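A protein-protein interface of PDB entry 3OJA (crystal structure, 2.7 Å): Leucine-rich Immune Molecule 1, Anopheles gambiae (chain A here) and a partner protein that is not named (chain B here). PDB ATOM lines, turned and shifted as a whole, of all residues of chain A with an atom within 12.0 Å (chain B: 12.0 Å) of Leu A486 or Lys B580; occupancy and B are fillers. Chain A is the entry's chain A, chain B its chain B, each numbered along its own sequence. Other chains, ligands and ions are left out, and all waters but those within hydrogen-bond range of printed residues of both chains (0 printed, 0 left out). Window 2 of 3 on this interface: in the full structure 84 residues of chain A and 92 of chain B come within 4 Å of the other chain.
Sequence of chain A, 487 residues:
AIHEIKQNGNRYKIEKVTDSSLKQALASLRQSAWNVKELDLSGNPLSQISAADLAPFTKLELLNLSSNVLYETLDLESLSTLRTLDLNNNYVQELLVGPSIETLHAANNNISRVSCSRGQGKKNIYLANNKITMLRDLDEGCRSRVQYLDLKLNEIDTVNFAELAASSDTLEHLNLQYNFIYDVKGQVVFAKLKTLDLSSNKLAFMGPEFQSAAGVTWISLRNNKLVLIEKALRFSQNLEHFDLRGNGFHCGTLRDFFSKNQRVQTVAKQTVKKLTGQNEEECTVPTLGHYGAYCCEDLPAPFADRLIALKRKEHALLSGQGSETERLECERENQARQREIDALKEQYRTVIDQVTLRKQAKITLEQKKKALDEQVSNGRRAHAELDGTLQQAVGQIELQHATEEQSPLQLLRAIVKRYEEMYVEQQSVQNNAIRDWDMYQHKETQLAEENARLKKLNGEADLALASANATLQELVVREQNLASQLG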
ATOM      1  N   VAL A 477       0.574  22.783  17.728  1.00  0.00           N
ATOM      2  CA  VAL A 477       1.307  23.714  18.562  1.00  0.00           C
ATOM      3  C   VAL A 477       0.473  24.037  19.822  1.00  0.00           C
ATOM      4  O   VAL A 477       1.007  24.125  20.923  1.00  0.00           O
ATOM      5  CB  VAL A 477       1.733  24.991  17.727  1.00  0.00           C
ATOM      6  CG1 VAL A 477       1.828  26.292  18.590  1.00  0.00           C
ATOM      7  CG2 VAL A 477       3.032  24.732  16.958  1.00  0.00           C
ATOM      8  N   ARG A 478      -0.844  24.162  19.670  1.00  0.00           N
ATOM      9  CA  ARG A 478      -1.717  24.443  20.808  1.00  0.00           C
ATOM     10  C   ARG A 478      -1.781  23.251  21.725  1.00  0.00           C
ATOM     11  O   ARG A 478      -2.201  23.374  22.844  1.00  0.00           O
ATOM     12  CB  ARG A 478      -3.142  24.785  20.378  1.00  0.00           C
ATOM     13  CG  ARG A 478      -3.307  26.177  19.878  1.00  0.00           C
ATOM     14  CD  ARG A 478      -4.665  26.365  19.190  1.00  0.00           C
ATOM     15  NE  ARG A 478      -5.763  26.180  20.133  1.00  0.00           N
ATOM     16  CZ  ARG A 478      -7.049  26.075  19.803  1.00  0.00           C
ATOM     17  NH1 ARG A 478      -7.432  26.121  18.531  1.00  0.00           N
ATOM     18  NH2 ARG A 478      -7.963  25.898  20.758  1.00  0.00           N
ATOM     19  N   GLU A 479      -1.408  22.079  21.261  1.00  0.00           N
ATOM     20  CA  GLU A 479      -1.532  20.932  22.115  1.00  0.00           C
ATOM     21  C   GLU A 479      -0.283  20.873  22.930  1.00  0.00           C
ATOM     22  O   GLU A 479      -0.312  20.634  24.113  1.00  0.00           O
ATOM     23  CB  GLU A 479      -1.689  19.662  21.331  1.00  0.00           C
ATOM     24  CG  GLU A 479      -1.811  18.471  22.199  1.00  0.00           C
ATOM     25  CD  GLU A 479      -1.512  17.243  21.436  1.00  0.00           C
ATOM     26  OE1 GLU A 479      -0.654  17.362  20.521  1.00  0.00           O
ATOM     27  OE2 GLU A 479      -2.133  16.188  21.720  1.00  0.00           O
ATOM     28  N   GLN A 480       0.844  21.128  22.317  1.00  0.00           N
ATOM     29  CA  GLN A 480       2.041  21.063  23.111  1.00  0.00           C
ATOM     30  C   GLN A 480       2.216  22.323  23.976  1.00  0.00           C
ATOM     31  O   GLN A 480       2.874  22.227  25.016  1.00  0.00           O
ATOM     32  CB  GLN A 480       3.274  20.712  22.274  1.00  0.00           C
ATOM     33  CG  GLN A 480       3.407  21.431  20.956  1.00  0.00           C
ATOM     34  CD  GLN A 480       4.261  20.660  19.932  1.00  0.00           C
ATOM     35  OE1 GLN A 480       4.237  19.402  19.864  1.00  0.00           O
ATOM     36  NE2 GLN A 480       5.024  21.421  19.119  1.00  0.00           N
ATOM     37  N   ASN A 481       1.605  23.468  23.628  1.00  0.00           N
ATOM     38  CA  ASN A 481       1.583  24.602  24.590  1.00  0.00           C
ATOM     39  C   ASN A 481       0.731  24.322  25.825  1.00  0.00           C
ATOM     40  O   ASN A 481       1.141  24.598  26.921  1.00  0.00           O
ATOM     41  CB  ASN A 481       1.178  25.929  23.953  1.00  0.00           C
ATOM     42  CG  ASN A 481       2.251  26.471  23.023  1.00  0.00           C
ATOM     43  OD1 ASN A 481       3.181  25.746  22.639  1.00  0.00           O
ATOM     44  ND2 ASN A 481       2.115  27.731  22.627  1.00  0.00           N
ATOM     45  N   LEU A 482      -0.434  23.738  25.659  1.00  0.00           N
ATOM     46  CA  LEU A 482      -1.220  23.397  26.817  1.00  0.00           C
ATOM     47  C   LEU A 482      -0.545  22.375  27.727  1.00  0.00           C
ATOM     48  O   LEU A 482      -0.666  22.427  28.936  1.00  0.00           O
ATOM     49  CB  LEU A 482      -2.586  22.859  26.390  1.00  0.00           C
ATOM     50  CG  LEU A 482      -3.409  23.978  25.786  1.00  0.00           C
ATOM     51  CD1 LEU A 482      -4.688  23.463  25.156  1.00  0.00           C
ATOM     52  CD2 LEU A 482      -3.723  24.975  26.819  1.00  0.00           C
ATOM     53  N   ALA A 483       0.132  21.406  27.160  1.00  0.00           N
ATOM     54  CA  ALA A 483       0.525  20.270  27.950  1.00  0.00           C
ATOM     55  C   ALA A 483       1.719  20.691  28.791  1.00  0.00           C
ATOM     56  O   ALA A 483       1.879  20.226  29.907  1.00  0.00           O
ATOM     57  CB  ALA A 483       0.861  19.118  27.054  1.00  0.00           C
ATOM     58  N   SER A 484       2.545  21.577  28.237  1.00  0.00           N
ATOM     59  CA  SER A 484       3.563  22.285  29.004  1.00  0.00           C
ATOM     60  C   SER A 484       2.912  22.969  30.204  1.00  0.00           C
ATOM     61  O   SER A 484       3.158  22.597  31.333  1.00  0.00           O
ATOM     62  CB  SER A 484       4.281  23.324  28.141  1.00  0.00           C
ATOM     63  OG  SER A 484       5.320  22.718  27.373  1.00  0.00           O
ATOM     64  N   GLN A 485       2.047  23.942  29.959  1.00  0.00           N
ATOM     65  CA  GLN A 485       1.350  24.643  31.028  1.00  0.00           C
ATOM     66  C   GLN A 485       0.719  23.758  32.092  1.00  0.00           C
ATOM     67  O   GLN A 485       0.469  24.217  33.195  1.00  0.00           O
ATOM     68  CB  GLN A 485       0.245  25.537  30.450  1.00  0.00           C
ATOM     69  CG  GLN A 485       0.752  26.672  29.555  1.00  0.00           C
ATOM     70  CD  GLN A 485      -0.383  27.444  28.827  1.00  0.00           C
ATOM     71  OE1 GLN A 485      -1.536  26.986  28.734  1.00  0.00           O
ATOM     72  NE2 GLN A 485      -0.038  28.627  28.308  1.00  0.00           N
ATOM     73  N   LEU A 486       0.434  22.508  31.793  1.00  0.00           N
ATOM     74  CA  LEU A 486      -0.610  21.847  32.567  1.00  0.00           C
ATOM     75  C   LEU A 486      -0.170  20.646  33.404  1.00  0.00           C
ATOM     76  O   LEU A 486      -0.819  20.293  34.392  1.00  0.00           O
ATOM     77  CB  LEU A 486      -1.774  21.469  31.656  1.00  0.00           C
ATOM     78  CG  LEU A 486      -3.040  21.127  32.421  1.00  0.00           C
ATOM     79  CD1 LEU A 486      -4.211  21.653  31.652  1.00  0.00           C
ATOM     80  CD2 LEU A 486      -3.169  19.596  32.696  1.00  0.00           C
ATOM     81  N   GLY A 487       0.925  20.015  33.025  1.00  0.00           N
ATOM     82  CA  GLY A 487       1.503  18.975  33.852  1.00  0.00           C
ATOM     83  C   GLY A 487       2.966  19.346  33.978  1.00  0.00           C
ATOM     84  O   GLY A 487       3.837  18.474  34.117  1.00  0.00           O
ATOM     85  OXT GLY A 487       3.310  20.540  33.908  1.00  0.00           O
ATOM     86  N   ARG B 571      -8.530  18.355  17.444  1.00  0.00           N
ATOM     87  CA  ARG B 571      -9.393  19.476  17.833  1.00  0.00           C
ATOM     88  C   ARG B 571     -10.013  19.054  19.144  1.00  0.00           C
ATOM     89  O   ARG B 571     -10.192  19.881  20.050  1.00  0.00           O
ATOM     90  CB  ARG B 571     -10.495  19.768  16.786  1.00  0.00           C
ATOM     91  CG  ARG B 571     -10.060  20.627  15.593  1.00  0.00           C
ATOM     92  CD  ARG B 571     -11.222  21.287  14.876  1.00  0.00           C
ATOM     93  NE  ARG B 571     -10.780  22.558  14.305  1.00  0.00           N
ATOM     94  CZ  ARG B 571     -10.585  22.802  12.990  1.00  0.00           C
ATOM     95  NH1 ARG B 571     -10.845  21.860  12.058  1.00  0.00           N
ATOM     96  NH2 ARG B 571     -10.154  24.010  12.576  1.00  0.00           N
ATOM     97  N   GLN B 572     -10.304  17.746  19.221  1.00  0.00           N
ATOM     98  CA  GLN B 572     -10.869  17.097  20.392  1.00  0.00           C
ATOM     99  C   GLN B 572      -9.854  17.096  21.545  1.00  0.00           C
ATOM    100  O   GLN B 572     -10.132  17.599  22.630  1.00  0.00           O
ATOM    101  CB  GLN B 572     -11.283  15.667  20.033  1.00  0.00           C
ATOM    102  CG  GLN B 572     -12.167  14.979  21.087  1.00  0.00           C
ATOM    103  CD  GLN B 572     -11.873  13.470  21.299  1.00  0.00           C
ATOM    104  OE1 GLN B 572     -10.697  13.018  21.315  1.00  0.00           O
ATOM    105  NE2 GLN B 572     -12.951  12.694  21.506  1.00  0.00           N
ATOM    106  N   LYS B 573      -8.680  16.529  21.304  1.00  0.00           N
ATOM    107  CA  LYS B 573      -7.615  16.521  22.289  1.00  0.00           C
ATOM    108  C   LYS B 573      -7.369  17.940  22.860  1.00  0.00           C
ATOM    109  O   LYS B 573      -7.180  18.092  24.062  1.00  0.00           O
ATOM    110  CB  LYS B 573      -6.335  15.962  21.645  1.00  0.00           C
ATOM    111  CG  LYS B 573      -5.180  15.573  22.592  1.00  0.00           C
ATOM    112  CD  LYS B 573      -5.302  14.125  23.091  1.00  0.00           C
ATOM    113  CE  LYS B 573      -3.936  13.522  23.502  1.00  0.00           C
ATOM    114  NZ  LYS B 573      -2.992  13.205  22.345  1.00  0.00           N
ATOM    115  N   VAL B 574      -7.377  18.974  22.018  1.00  0.00           N
ATOM    116  CA  VAL B 574      -7.099  20.329  22.484  1.00  0.00           C
ATOM    117  C   VAL B 574      -8.265  20.919  23.249  1.00  0.00           C
ATOM    118  O   VAL B 574      -8.083  21.767  24.103  1.00  0.00           O
ATOM    119  CB  VAL B 574      -6.744  21.246  21.349  1.00  0.00           C
ATOM    120  CG1 VAL B 574      -6.930  22.689  21.722  1.00  0.00           C
ATOM    121  CG2 VAL B 574      -5.325  21.003  20.958  1.00  0.00           C
ATOM    122  N   LYS B 575      -9.475  20.477  22.955  1.00  0.00           N
ATOM    123  CA  LYS B 575     -10.623  20.923  23.722  1.00  0.00           C
ATOM    124  C   LYS B 575     -10.500  20.286  25.112  1.00  0.00           C
ATOM    125  O   LYS B 575     -10.649  20.973  26.118  1.00  0.00           O
ATOM    126  CB  LYS B 575     -11.935  20.528  23.026  1.00  0.00           C
ATOM    127  CG  LYS B 575     -13.168  21.262  23.550  1.00  0.00           C
ATOM    128  CD  LYS B 575     -14.436  20.877  22.807  1.00  0.00           C
ATOM    129  CE  LYS B 575     -14.272  20.992  21.293  1.00  0.00           C
ATOM    130  NZ  LYS B 575     -15.511  20.551  20.573  1.00  0.00           N
ATOM    131  N   GLN B 576     -10.184  18.989  25.167  1.00  0.00           N
ATOM    132  CA  GLN B 576      -9.989  18.308  26.446  1.00  0.00           C
ATOM    133  C   GLN B 576      -8.886  18.986  27.276  1.00  0.00           C
ATOM    134  O   GLN B 576      -9.030  19.140  28.465  1.00  0.00           O
ATOM    135  CB  GLN B 576      -9.658  16.812  26.268  1.00  0.00           C
ATOM    136  CG  GLN B 576     -10.846  15.886  25.923  1.00  0.00           C
ATOM    137  CD  GLN B 576     -10.403  14.430  25.626  1.00  0.00           C
ATOM    138  OE1 GLN B 576      -9.604  14.183  24.711  1.00  0.00           O
ATOM    139  NE2 GLN B 576     -10.921  13.469  26.403  1.00  0.00           N
ATOM    140  N   LEU B 577      -7.782  19.391  26.664  1.00  0.00           N
ATOM    141  CA  LEU B 577      -6.706  20.006  27.433  1.00  0.00           C
ATOM    142  C   LEU B 577      -7.142  21.359  27.961  1.00  0.00           C
ATOM    143  O   LEU B 577      -6.535  21.884  28.879  1.00  0.00           O
ATOM    144  CB  LEU B 577      -5.416  20.149  26.615  1.00  0.00           C
ATOM    145  CG  LEU B 577      -4.702  18.827  26.336  1.00  0.00           C
ATOM    146  CD1 LEU B 577      -3.385  19.114  25.648  1.00  0.00           C
ATOM    147  CD2 LEU B 577      -4.463  17.990  27.595  1.00  0.00           C
ATOM    148  N   GLU B 578      -8.201  21.932  27.410  1.00  0.00           N
ATOM    149  CA  GLU B 578      -8.599  23.260  27.875  1.00  0.00           C
ATOM    150  C   GLU B 578      -9.550  23.208  29.077  1.00  0.00           C
ATOM    151  O   GLU B 578      -9.457  24.048  29.979  1.00  0.00           O
ATOM    152  CB  GLU B 578      -9.097  24.145  26.726  1.00  0.00           C
ATOM    153  CG  GLU B 578      -7.897  24.674  25.934  1.00  0.00           C
ATOM    154  CD  GLU B 578      -8.242  25.468  24.688  1.00  0.00           C
ATOM    155  OE1 GLU B 578      -9.274  25.188  24.023  1.00  0.00           O
ATOM    156  OE2 GLU B 578      -7.436  26.370  24.359  1.00  0.00           O
ATOM    157  N   ALA B 579     -10.406  22.189  29.115  1.00  0.00           N
ATOM    158  CA  ALA B 579     -11.296  21.969  30.262  1.00  0.00           C
ATOM    159  C   ALA B 579     -10.477  21.608  31.494  1.00  0.00           C
ATOM    160  O   ALA B 579     -10.836  21.950  32.619  1.00  0.00           O
ATOM    161  CB  ALA B 579     -12.307  20.848  29.961  1.00  0.00           C
ATOM    162  N   LYS B 580      -9.384  20.894  31.252  1.00  0.00           N
ATOM    163  CA  LYS B 580      -8.497  20.385  32.279  1.00  0.00           C
ATOM    164  C   LYS B 580      -7.615  21.564  32.666  1.00  0.00           C
ATOM    165  O   LYS B 580      -6.632  21.431  33.372  1.00  0.00           O
ATOM    166  CB  LYS B 580      -7.699  19.215  31.683  1.00  0.00           C
ATOM    167  CG  LYS B 580      -6.699  18.483  32.575  1.00  0.00           C
ATOM    168  CD  LYS B 580      -7.359  17.606  33.619  1.00  0.00           C
ATOM    169  CE  LYS B 580      -6.320  17.091  34.642  1.00  0.00           C
ATOM    170  NZ  LYS B 580      -6.920  16.631  35.954  1.00  0.00           N
ATOM    171  N   LYS B 581      -7.981  22.742  32.185  1.00  0.00           N
ATOM    172  CA  LYS B 581      -7.321  23.975  32.584  1.00  0.00           C
ATOM    173  C   LYS B 581      -8.408  24.997  32.927  1.00  0.00           C
ATOM    174  O   LYS B 581      -8.136  26.186  33.045  1.00  0.00           O
ATOM    175  CB  LYS B 581      -6.449  24.472  31.436  1.00  0.00           C
ATOM    176  CG  LYS B 581      -5.736  25.764  31.676  1.00  0.00           C
ATOM    177  CD  LYS B 581      -4.985  26.190  30.449  1.00  0.00           C
ATOM    178  CE  LYS B 581      -4.342  27.554  30.631  1.00  0.00           C
ATOM    179  NZ  LYS B 581      -3.302  27.517  31.719  1.00  0.00           N
ATOM    180  N   ASN B 582      -9.644  24.508  33.066  1.00  0.00           N
ATOM    181  CA  ASN B 582     -10.816  25.302  33.477  1.00  0.00           C
ATOM    182  C   ASN B 582     -10.860  26.714  32.860  1.00  0.00           C
ATOM    183  O   ASN B 582     -10.593  26.913  31.662  1.00  0.00           O
ATOM    184  CB  ASN B 582     -10.893  25.361  35.021  1.00  0.00           C
ATOM    185  CG  ASN B 582     -10.952  23.935  35.696  1.00  0.00           C
ATOM    186  OD1 ASN B 582     -11.965  23.211  35.613  1.00  0.00           O
ATOM    187  ND2 ASN B 582      -9.864  23.562  36.386  1.00  0.00           N
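Leu A486 touches just these residues of chain B: Leu B577 (3.6 Å), Lys B580 (3.0 Å) and Lys B581 (3.6 Å).
Of chain A, only Leu A486 (3.0 Å) comes within 4 Å of Lys B580.
No residue of chain B comes within 4 Å of Ala A483.
No residue of chain B comes within 4 Å of Ser A484.
No residue of chain B comes within 4 Å of Gly A487.
Leu B577 touches just these residues of chain A: Glu A479 (3.8 Å), Leu A482 (3.7 Å) and Leu A486 (3.6 Å).
No residue of chain A comes within 4 Å of Ala B579.
Of the printed residues of chain A, Val B574 touches Arg A478 (3.5 Å), Glu A479 (3.9 Å) and Leu A482 (3.9 Å).
Of the printed residues of chain A, Lys B573 touches Glu A479.
Printed residues of chain B within 4 Å of Glu A479: Lys B573 (3.2 Å), Val B574 (3.9 Å) and Leu B577 (3.8 Å).
Gln B576 touches none of the printed residues of chain A.
The nearest residue of chain A that does not touch Lys B580 is Leu A482 (7.5 Å).
Printed residues of chain A that touch a printed residue of chain B: Arg A478, Glu A479, Leu A482, Gln A485 and Leu A486.
Hydrophobic or aromatic side chains of chain A within 4 Å of the printed part of chain B: Leu A482 and Leu A486.
Of the 12 printed residues of chain B, 6 touch a printed residue of chain A.
Printed residues of chain B that touch a printed residue of chain A: Lys B573, Val B574, Leu B577, Glu B578, Lys B580 and Lys B581.
Hydrophobic or aromatic side chains of chain B that line the printed part of chain A: Val B574 and Leu B577.
Among the printed residues, Asp or Glu carboxylates within 4 Å of a Lys or Arg side-chain nitrogen of the other chain: Arg A478 with Glu B578 and Glu A479 with Lys B573.
NH2 of Arg A478 is in salt-bridge range of OE1 of Glu B578 (3.6 Å).
The side-chain carboxylate (OE2) of Glu A479 lies within salt-bridge range of the side-chain amino group (NZ) of Lys B573 (3.2 Å).
Arg A478 touches Val B574 (NH2 to CG1, 3.5 Å).
CG2 of Val B574 touches CB of Glu A479 (3.9 Å).
CD1 of Leu B577 touches O of Glu A479, at 3.8 Å.
Leu A482 touches Val B574.
CB of Leu B577 touches CD1 of Leu A482, 3.7 Å away.
Leu A482 touches Glu B578 (CD1 to CG, 3.5 Å).
Gln A485 touches Lys B581 (OE1 to CE, 3.4 Å).
Leu A486 touches Leu B577 (CD1 to O, 3.6 Å).
CD1 of Leu A486 touches O of Lys B580 (3.0 Å).
Leu A486 touches Lys B581.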
